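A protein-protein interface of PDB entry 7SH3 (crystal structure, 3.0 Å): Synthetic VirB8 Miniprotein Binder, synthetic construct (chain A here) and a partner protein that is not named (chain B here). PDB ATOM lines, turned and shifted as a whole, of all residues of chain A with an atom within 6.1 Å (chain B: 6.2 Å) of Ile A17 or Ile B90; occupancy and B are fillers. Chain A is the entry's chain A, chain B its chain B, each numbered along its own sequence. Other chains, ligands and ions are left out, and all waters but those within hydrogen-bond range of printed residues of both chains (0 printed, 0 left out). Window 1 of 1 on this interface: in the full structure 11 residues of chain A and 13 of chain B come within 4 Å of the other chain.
Among the printed residues, merely in contact across the chains: Gly A16 with Ile B90 (3.4 Å), Ile A17 with Leu B65 (3.6 Å), Ile A17 with Met B88 (3.0 Å), Ile A17 with Ile B90 (3.4 Å), Ile A17 with Val B97 (3.6 Å), Trp A20 with Ile B90 (3.8 Å), Trp A20 with Ile B98 (3.98 Å), Leu A21 with Val B97 (3.6 Å), Val A32 with Ile B90 (3.9 Å), Asn A36 with Ile B90 (3.3 Å) and Asn A36 with Asp B91 (3.6 Å).
The side-chain hydroxyl (OG1) of Thr A13 is in hydrogen-bond range of the side-chain amide nitrogen (ND2) of Asn B89.
OD1 of Asn B89 is in hydrogen-bond range of ND2 of Asn A36 (2.9 Å).
Of the printed residues of chain B, Ile A17 touches Leu B65 (3.6 Å), Met B88 (3.0 Å), Ile B90 (3.4 Å) and Val B97 (3.6 Å).
Of chain A, only Gly A16 (3.4 Å), Ile A17 (3.4 Å), Trp A20 (3.8 Å), Val A32 (3.9 Å) and Asn A36 (3.3 Å) come within 4 Å of Ile B90.
Of the printed residues of chain B, Val A32 touches Ile B90.
Of the printed residues of chain B, Leu A21 touches Val B97.
Of the printed residues of chain B, Thr A13 touches Asn B89.
Printed residues of chain B within 4 Å of Gly A16: Ile B90 (3.4 Å).
Leu A22 touches none of the printed residues of chain B.
The nearest residue of chain A that does not touch Ile B90 is Arg A33 (4.3 Å).
The nearest printed residue of chain B that does not touch Gly A16 is Asn B89 (5.9 Å).
Hydrophobic or aromatic side chains of chain B within 4 Å of the printed part of chain A: Leu B65, Ile B90, Val B97 and Ile B98.
Among the printed residues, 13 pairs touch across the chains.
OG of Ser B95 lies within hydrogen-bond range of O of Met B88.
The side-chain hydroxyl (OG) of Ser B95 sits at hydrogen-bond distance from the backbone NH (N) of Val B97 (3.0 Å).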
ATOM      1  N   ALA A  12      23.748  31.700  -2.285  1.00  0.00           N
ATOM      2  CA  ALA A  12      24.785  30.739  -1.905  1.00  0.00           C
ATOM      3  C   ALA A  12      24.263  29.690  -0.932  1.00  0.00           C
ATOM      4  O   ALA A  12      24.749  28.549  -0.924  1.00  0.00           O
ATOM      5  CB  ALA A  12      25.977  31.465  -1.285  1.00  0.00           C
ATOM      6  N   THR A  13      23.295  30.067  -0.091  1.00  0.00           N
ATOM      7  CA  THR A  13      22.734  29.132   0.874  1.00  0.00           C
ATOM      8  C   THR A  13      21.993  28.020   0.170  1.00  0.00           C
ATOM      9  O   THR A  13      22.269  26.841   0.404  1.00  0.00           O
ATOM     10  CB  THR A  13      21.808  29.856   1.847  1.00  0.00           C
ATOM     11  OG1 THR A  13      22.591  30.724   2.688  1.00  0.00           O
ATOM     12  CG2 THR A  13      21.019  28.839   2.714  1.00  0.00           C
ATOM     13  N   LEU A  14      21.053  28.385  -0.705  1.00  0.00           N
ATOM     14  CA  LEU A  14      20.429  27.418  -1.604  1.00  0.00           C
ATOM     15  C   LEU A  14      21.467  26.558  -2.321  1.00  0.00           C
ATOM     16  O   LEU A  14      21.520  25.348  -2.109  1.00  0.00           O
ATOM     17  CB  LEU A  14      19.533  28.154  -2.602  1.00  0.00           C
ATOM     18  CG  LEU A  14      18.586  27.320  -3.464  1.00  0.00           C
ATOM     19  CD1 LEU A  14      17.883  26.300  -2.627  1.00  0.00           C
ATOM     20  CD2 LEU A  14      17.545  28.246  -4.109  1.00  0.00           C
ATOM     21  N   VAL A  15      22.308  27.175  -3.162  1.00  0.00           N
ATOM     22  CA  VAL A  15      23.384  26.461  -3.852  1.00  0.00           C
ATOM     23  C   VAL A  15      24.096  25.498  -2.907  1.00  0.00           C
ATOM     24  O   VAL A  15      24.267  24.308  -3.209  1.00  0.00           O
ATOM     25  CB  VAL A  15      24.376  27.462  -4.476  1.00  0.00           C
ATOM     26  CG1 VAL A  15      25.629  26.743  -4.987  1.00  0.00           C
ATOM     27  CG2 VAL A  15      23.717  28.254  -5.596  1.00  0.00           C
ATOM     28  N   GLY A  16      24.510  25.995  -1.739  1.00  0.00           N
ATOM     29  CA  GLY A  16      25.252  25.151  -0.815  1.00  0.00           C
ATOM     30  C   GLY A  16      24.433  24.000  -0.264  1.00  0.00           C
ATOM     31  O   GLY A  16      24.983  22.940   0.046  1.00  0.00           O
ATOM     32  N   ILE A  17      23.119  24.200  -0.115  1.00  0.00           N
ATOM     33  CA  ILE A  17      22.227  23.093   0.213  1.00  0.00           C
ATOM     34  C   ILE A  17      22.291  22.028  -0.876  1.00  0.00           C
ATOM     35  O   ILE A  17      22.676  20.877  -0.625  1.00  0.00           O
ATOM     36  CB  ILE A  17      20.783  23.588   0.413  1.00  0.00           C
ATOM     37  CG1 ILE A  17      20.669  24.517   1.628  1.00  0.00           C
ATOM     38  CG2 ILE A  17      19.837  22.404   0.545  1.00  0.00           C
ATOM     39  CD1 ILE A  17      21.624  24.161   2.726  1.00  0.00           C
ATOM     40  N   GLU A  18      21.924  22.400  -2.111  1.00  0.00           N
ATOM     41  CA  GLU A  18      21.779  21.384  -3.150  1.00  0.00           C
ATOM     42  C   GLU A  18      23.092  20.675  -3.432  1.00  0.00           C
ATOM     43  O   GLU A  18      23.088  19.578  -3.996  1.00  0.00           O
ATOM     44  CB  GLU A  18      21.274  21.976  -4.464  1.00  0.00           C
ATOM     45  CG  GLU A  18      19.949  22.708  -4.391  1.00  0.00           C
ATOM     46  CD  GLU A  18      19.722  23.541  -5.635  1.00  0.00           C
ATOM     47  OE1 GLU A  18      20.543  24.434  -5.915  1.00  0.00           O
ATOM     48  OE2 GLU A  18      18.693  23.332  -6.311  1.00  0.00           O
ATOM     49  N   ALA A  19      24.216  21.291  -3.090  1.00  0.00           N
ATOM     50  CA  ALA A  19      25.479  20.577  -3.191  1.00  0.00           C
ATOM     51  C   ALA A  19      25.614  19.598  -2.031  1.00  0.00           C
ATOM     52  O   ALA A  19      25.948  18.428  -2.237  1.00  0.00           O
ATOM     53  CB  ALA A  19      26.648  21.571  -3.246  1.00  0.00           C
ATOM     54  N   TRP A  20      25.305  20.054  -0.808  1.00  0.00           N
ATOM     55  CA  TRP A  20      25.323  19.154   0.339  1.00  0.00           C
ATOM     56  C   TRP A  20      24.469  17.907   0.101  1.00  0.00           C
ATOM     57  O   TRP A  20      24.888  16.785   0.418  1.00  0.00           O
ATOM     58  CB  TRP A  20      24.868  19.888   1.602  1.00  0.00           C
ATOM     59  CG  TRP A  20      24.836  18.952   2.775  1.00  0.00           C
ATOM     60  CD1 TRP A  20      23.773  18.167   3.178  1.00  0.00           C
ATOM     61  CD2 TRP A  20      25.928  18.617   3.640  1.00  0.00           C
ATOM     62  NE1 TRP A  20      24.133  17.402   4.263  1.00  0.00           N
ATOM     63  CE2 TRP A  20      25.449  17.652   4.566  1.00  0.00           C
ATOM     64  CE3 TRP A  20      27.256  19.045   3.736  1.00  0.00           C
ATOM     65  CZ2 TRP A  20      26.258  17.117   5.575  1.00  0.00           C
ATOM     66  CZ3 TRP A  20      28.056  18.510   4.737  1.00  0.00           C
ATOM     67  CH2 TRP A  20      27.551  17.557   5.644  1.00  0.00           C
ATOM     68  N   LEU A  21      23.282  18.081  -0.478  1.00  0.00           N
ATOM     69  CA  LEU A  21      22.349  16.970  -0.589  1.00  0.00           C
ATOM     70  C   LEU A  21      22.832  15.920  -1.576  1.00  0.00           C
ATOM     71  O   LEU A  21      22.627  14.720  -1.356  1.00  0.00           O
ATOM     72  CB  LEU A  21      20.976  17.494  -0.983  1.00  0.00           C
ATOM     73  CG  LEU A  21      20.322  18.111   0.242  1.00  0.00           C
ATOM     74  CD1 LEU A  21      18.969  18.703  -0.108  1.00  0.00           C
ATOM     75  CD2 LEU A  21      20.201  17.044   1.329  1.00  0.00           C
ATOM     76  N   LEU A  22      23.481  16.349  -2.656  1.00  0.00           N
ATOM     77  CA  LEU A  22      23.931  15.481  -3.737  1.00  0.00           C
ATOM     78  C   LEU A  22      25.276  14.820  -3.477  1.00  0.00           C
ATOM     79  O   LEU A  22      25.689  13.969  -4.277  1.00  0.00           O
ATOM     80  CB  LEU A  22      24.010  16.302  -5.026  1.00  0.00           C
ATOM     81  CG  LEU A  22      22.729  16.753  -5.712  1.00  0.00           C
ATOM     82  CD1 LEU A  22      22.998  17.594  -6.952  1.00  0.00           C
ATOM     83  CD2 LEU A  22      22.047  15.461  -6.129  1.00  0.00           C
ATOM     84  N   VAL A  32      31.965  21.031   0.116  1.00  0.00           N
ATOM     85  CA  VAL A  32      30.777  21.882   0.088  1.00  0.00           C
ATOM     86  C   VAL A  32      30.617  22.629   1.409  1.00  0.00           C
ATOM     87  O   VAL A  32      30.263  23.816   1.435  1.00  0.00           O
ATOM     88  CB  VAL A  32      29.543  21.026  -0.241  1.00  0.00           C
ATOM     89  CG1 VAL A  32      28.303  21.824  -0.145  1.00  0.00           C
ATOM     90  CG2 VAL A  32      29.666  20.486  -1.633  1.00  0.00           C
ATOM     91  N   ARG A  33      30.895  21.957   2.525  1.00  0.00           N
ATOM     92  CA  ARG A  33      30.779  22.603   3.826  1.00  0.00           C
ATOM     93  C   ARG A  33      31.773  23.755   3.964  1.00  0.00           C
ATOM     94  O   ARG A  33      31.446  24.802   4.529  1.00  0.00           O
ATOM     95  CB  ARG A  33      30.966  21.543   4.916  1.00  0.00           C
ATOM     96  CG  ARG A  33      31.230  22.009   6.336  1.00  0.00           C
ATOM     97  CD  ARG A  33      32.087  20.961   7.034  1.00  0.00           C
ATOM     98  NE  ARG A  33      31.560  19.619   6.797  1.00  0.00           N
ATOM     99  CZ  ARG A  33      32.247  18.496   6.967  1.00  0.00           C
ATOM    100  NH1 ARG A  33      33.447  18.498   7.521  1.00  0.00           N
ATOM    101  NH2 ARG A  33      31.713  17.338   6.580  1.00  0.00           N
ATOM    102  N   ASN A  36      30.892  26.695   1.469  1.00  0.00           N
ATOM    103  CA  ASN A  36      29.722  27.369   2.019  1.00  0.00           C
ATOM    104  C   ASN A  36      30.123  28.312   3.147  1.00  0.00           C
ATOM    105  O   ASN A  36      29.789  29.499   3.124  1.00  0.00           O
ATOM    106  CB  ASN A  36      28.722  26.318   2.501  1.00  0.00           C
ATOM    107  CG  ASN A  36      27.481  26.911   3.103  1.00  0.00           C
ATOM    108  OD1 ASN A  36      26.660  27.498   2.400  1.00  0.00           O
ATOM    109  ND2 ASN A  36      27.316  26.736   4.408  1.00  0.00           N
ATOM    110  N   TYR B  60       9.213  20.488   4.734  1.00  0.00           N
ATOM    111  CA  TYR B  60      10.508  20.065   4.197  1.00  0.00           C
ATOM    112  C   TYR B  60      10.217  18.988   3.168  1.00  0.00           C
ATOM    113  O   TYR B  60       9.962  17.843   3.531  1.00  0.00           O
ATOM    114  CB  TYR B  60      11.450  19.513   5.256  1.00  0.00           C
ATOM    115  CG  TYR B  60      12.784  19.118   4.661  1.00  0.00           C
ATOM    116  CD1 TYR B  60      13.734  20.086   4.314  1.00  0.00           C
ATOM    117  CD2 TYR B  60      13.076  17.785   4.371  1.00  0.00           C
ATOM    118  CE1 TYR B  60      14.955  19.731   3.755  1.00  0.00           C
ATOM    119  CE2 TYR B  60      14.299  17.423   3.802  1.00  0.00           C
ATOM    120  CZ  TYR B  60      15.230  18.399   3.499  1.00  0.00           C
ATOM    121  OH  TYR B  60      16.428  18.033   2.939  1.00  0.00           O
ATOM    122  N   LEU B  65      12.804  22.618  -2.611  1.00  0.00           N
ATOM    123  CA  LEU B  65      13.454  23.714  -1.904  1.00  0.00           C
ATOM    124  C   LEU B  65      13.490  24.983  -2.750  1.00  0.00           C
ATOM    125  O   LEU B  65      13.305  26.092  -2.232  1.00  0.00           O
ATOM    126  CB  LEU B  65      14.854  23.278  -1.478  1.00  0.00           C
ATOM    127  CG  LEU B  65      14.880  22.347  -0.264  1.00  0.00           C
ATOM    128  CD1 LEU B  65      16.287  22.026   0.172  1.00  0.00           C
ATOM    129  CD2 LEU B  65      14.154  23.002   0.877  1.00  0.00           C
ATOM    130  N   PHE B  69      11.883  28.382  -1.282  1.00  0.00           N
ATOM    131  CA  PHE B  69      12.666  29.614  -1.316  1.00  0.00           C
ATOM    132  C   PHE B  69      11.991  30.687  -2.158  1.00  0.00           C
ATOM    133  O   PHE B  69      11.780  31.811  -1.695  1.00  0.00           O
ATOM    134  CB  PHE B  69      14.051  29.289  -1.872  1.00  0.00           C
ATOM    135  CG  PHE B  69      15.046  28.889  -0.822  1.00  0.00           C
ATOM    136  CD1 PHE B  69      14.930  27.670  -0.161  1.00  0.00           C
ATOM    137  CD2 PHE B  69      16.134  29.688  -0.543  1.00  0.00           C
ATOM    138  CE1 PHE B  69      15.860  27.291   0.801  1.00  0.00           C
ATOM    139  CE2 PHE B  69      17.074  29.308   0.410  1.00  0.00           C
ATOM    140  CZ  PHE B  69      16.937  28.112   1.080  1.00  0.00           C
ATOM    141  N   PHE B  87      18.668  29.915   8.406  1.00  0.00           N
ATOM    142  CA  PHE B  87      18.275  28.725   9.145  1.00  0.00           C
ATOM    143  C   PHE B  87      18.469  27.452   8.337  1.00  0.00           C
ATOM    144  O   PHE B  87      18.887  26.430   8.893  1.00  0.00           O
ATOM    145  CB  PHE B  87      16.809  28.851   9.590  1.00  0.00           C
ATOM    146  CG  PHE B  87      16.316  27.692  10.413  1.00  0.00           C
ATOM    147  CD1 PHE B  87      16.888  27.402  11.643  1.00  0.00           C
ATOM    148  CD2 PHE B  87      15.258  26.919   9.974  1.00  0.00           C
ATOM    149  CE1 PHE B  87      16.447  26.344  12.407  1.00  0.00           C
ATOM    150  CE2 PHE B  87      14.799  25.850  10.731  1.00  0.00           C
ATOM    151  CZ  PHE B  87      15.393  25.566  11.956  1.00  0.00           C
ATOM    152  N   MET B  88      18.210  27.515   7.031  1.00  0.00           N
ATOM    153  CA  MET B  88      18.376  26.397   6.118  1.00  0.00           C
ATOM    154  C   MET B  88      19.834  26.156   5.713  1.00  0.00           C
ATOM    155  O   MET B  88      20.143  25.080   5.199  1.00  0.00           O
ATOM    156  CB  MET B  88      17.534  26.651   4.860  1.00  0.00           C
ATOM    157  CG  MET B  88      16.060  26.983   5.122  1.00  0.00           C
ATOM    158  SD  MET B  88      15.047  25.622   5.773  1.00  0.00           S
ATOM    159  CE  MET B  88      14.537  24.781   4.281  1.00  0.00           C
ATOM    160  N   ASN B  89      20.725  27.127   5.919  1.00  0.00           N
ATOM    161  CA  ASN B  89      22.120  26.995   5.514  1.00  0.00           C
ATOM    162  C   ASN B  89      22.765  25.820   6.246  1.00  0.00           C
ATOM    163  O   ASN B  89      22.439  25.536   7.402  1.00  0.00           O
ATOM    164  CB  ASN B  89      22.856  28.311   5.819  1.00  0.00           C
ATOM    165  CG  ASN B  89      24.102  28.532   4.954  1.00  0.00           C
ATOM    166  OD1 ASN B  89      25.223  28.531   5.445  1.00  0.00           O
ATOM    167  ND2 ASN B  89      23.900  28.768   3.681  1.00  0.00           N
ATOM    168  N   ILE B  90      23.652  25.102   5.552  1.00  0.00           N
ATOM    169  CA  ILE B  90      24.264  23.924   6.157  1.00  0.00           C
ATOM    170  C   ILE B  90      25.294  24.299   7.208  1.00  0.00           C
ATOM    171  O   ILE B  90      25.862  23.412   7.858  1.00  0.00           O
ATOM    172  CB  ILE B  90      24.911  23.009   5.099  1.00  0.00           C
ATOM    173  CG1 ILE B  90      25.736  23.820   4.100  1.00  0.00           C
ATOM    174  CG2 ILE B  90      23.853  22.224   4.392  1.00  0.00           C
ATOM    175  CD1 ILE B  90      26.527  22.980   3.118  1.00  0.00           C
ATOM    176  N   ASP B  91      25.554  25.604   7.360  1.00  0.00           N
ATOM    177  CA  ASP B  91      26.300  26.140   8.493  1.00  0.00           C
ATOM    178  C   ASP B  91      25.566  25.830   9.791  1.00  0.00           C
ATOM    179  O   ASP B  91      26.200  25.552  10.814  1.00  0.00           O
ATOM    180  CB  ASP B  91      26.463  27.656   8.276  1.00  0.00           C
ATOM    181  CG  ASP B  91      27.059  28.409   9.472  1.00  0.00           C
ATOM    182  OD1 ASP B  91      27.430  27.784  10.485  1.00  0.00           O
ATOM    183  OD2 ASP B  91      27.114  29.655   9.399  1.00  0.00           O
ATOM    184  N   ASN B  92      24.231  25.826   9.743  1.00  0.00           N
ATOM    185  CA  ASN B  92      23.383  25.570  10.906  1.00  0.00           C
ATOM    186  C   ASN B  92      23.256  24.085  11.221  1.00  0.00           C
ATOM    187  O   ASN B  92      22.878  23.288  10.358  1.00  0.00           O
ATOM    188  CB  ASN B  92      21.990  26.152  10.674  1.00  0.00           C
ATOM    189  CG  ASN B  92      21.117  26.035  11.894  1.00  0.00           C
ATOM    190  OD1 ASN B  92      21.611  26.088  13.022  1.00  0.00           O
ATOM    191  ND2 ASN B  92      19.812  25.883  11.684  1.00  0.00           N
ATOM    192  N   SER B  93      23.532  23.727  12.481  1.00  0.00           N
ATOM    193  CA  SER B  93      23.454  22.332  12.904  1.00  0.00           C
ATOM    194  C   SER B  93      22.016  21.833  12.924  1.00  0.00           C
ATOM    195  O   SER B  93      21.758  20.652  12.662  1.00  0.00           O
ATOM    196  CB  SER B  93      24.084  22.178  14.287  1.00  0.00           C
ATOM    197  OG  SER B  93      25.488  22.359  14.222  1.00  0.00           O
ATOM    198  N   SER B  95      19.597  22.750  10.943  1.00  0.00           N
ATOM    199  CA  SER B  95      18.896  22.899   9.684  1.00  0.00           C
ATOM    200  C   SER B  95      18.169  21.599   9.350  1.00  0.00           C
ATOM    201  O   SER B  95      18.585  20.520   9.781  1.00  0.00           O
ATOM    202  CB  SER B  95      19.866  23.263   8.566  1.00  0.00           C
ATOM    203  OG  SER B  95      19.351  22.852   7.314  1.00  0.00           O
ATOM    204  N   VAL B  97      17.989  20.344   6.332  1.00  0.00           N
ATOM    205  CA  VAL B  97      18.829  19.681   5.341  1.00  0.00           C
ATOM    206  C   VAL B  97      19.860  18.788   6.016  1.00  0.00           C
ATOM    207  O   VAL B  97      20.132  17.675   5.556  1.00  0.00           O
ATOM    208  CB  VAL B  97      19.482  20.733   4.432  1.00  0.00           C
ATOM    209  CG1 VAL B  97      20.209  20.070   3.319  1.00  0.00           C
ATOM    210  CG2 VAL B  97      18.404  21.638   3.863  1.00  0.00           C
ATOM    211  N   ILE B  98      20.445  19.250   7.119  1.00  0.00           N
ATOM    212  CA  ILE B  98      21.395  18.416   7.848  1.00  0.00           C
ATOM    213  C   ILE B  98      20.680  17.230   8.486  1.00  0.00           C
ATOM    214  O   ILE B  98      21.083  16.077   8.309  1.00  0.00           O
ATOM    215  CB  ILE B  98      22.131  19.245   8.910  1.00  0.00           C
ATOM    216  CG1 ILE B  98      22.963  20.340   8.247  1.00  0.00           C
ATOM    217  CG2 ILE B  98      22.991  18.314   9.774  1.00  0.00           C
ATOM    218  CD1 ILE B  98      24.298  19.869   7.686  1.00  0.00           C
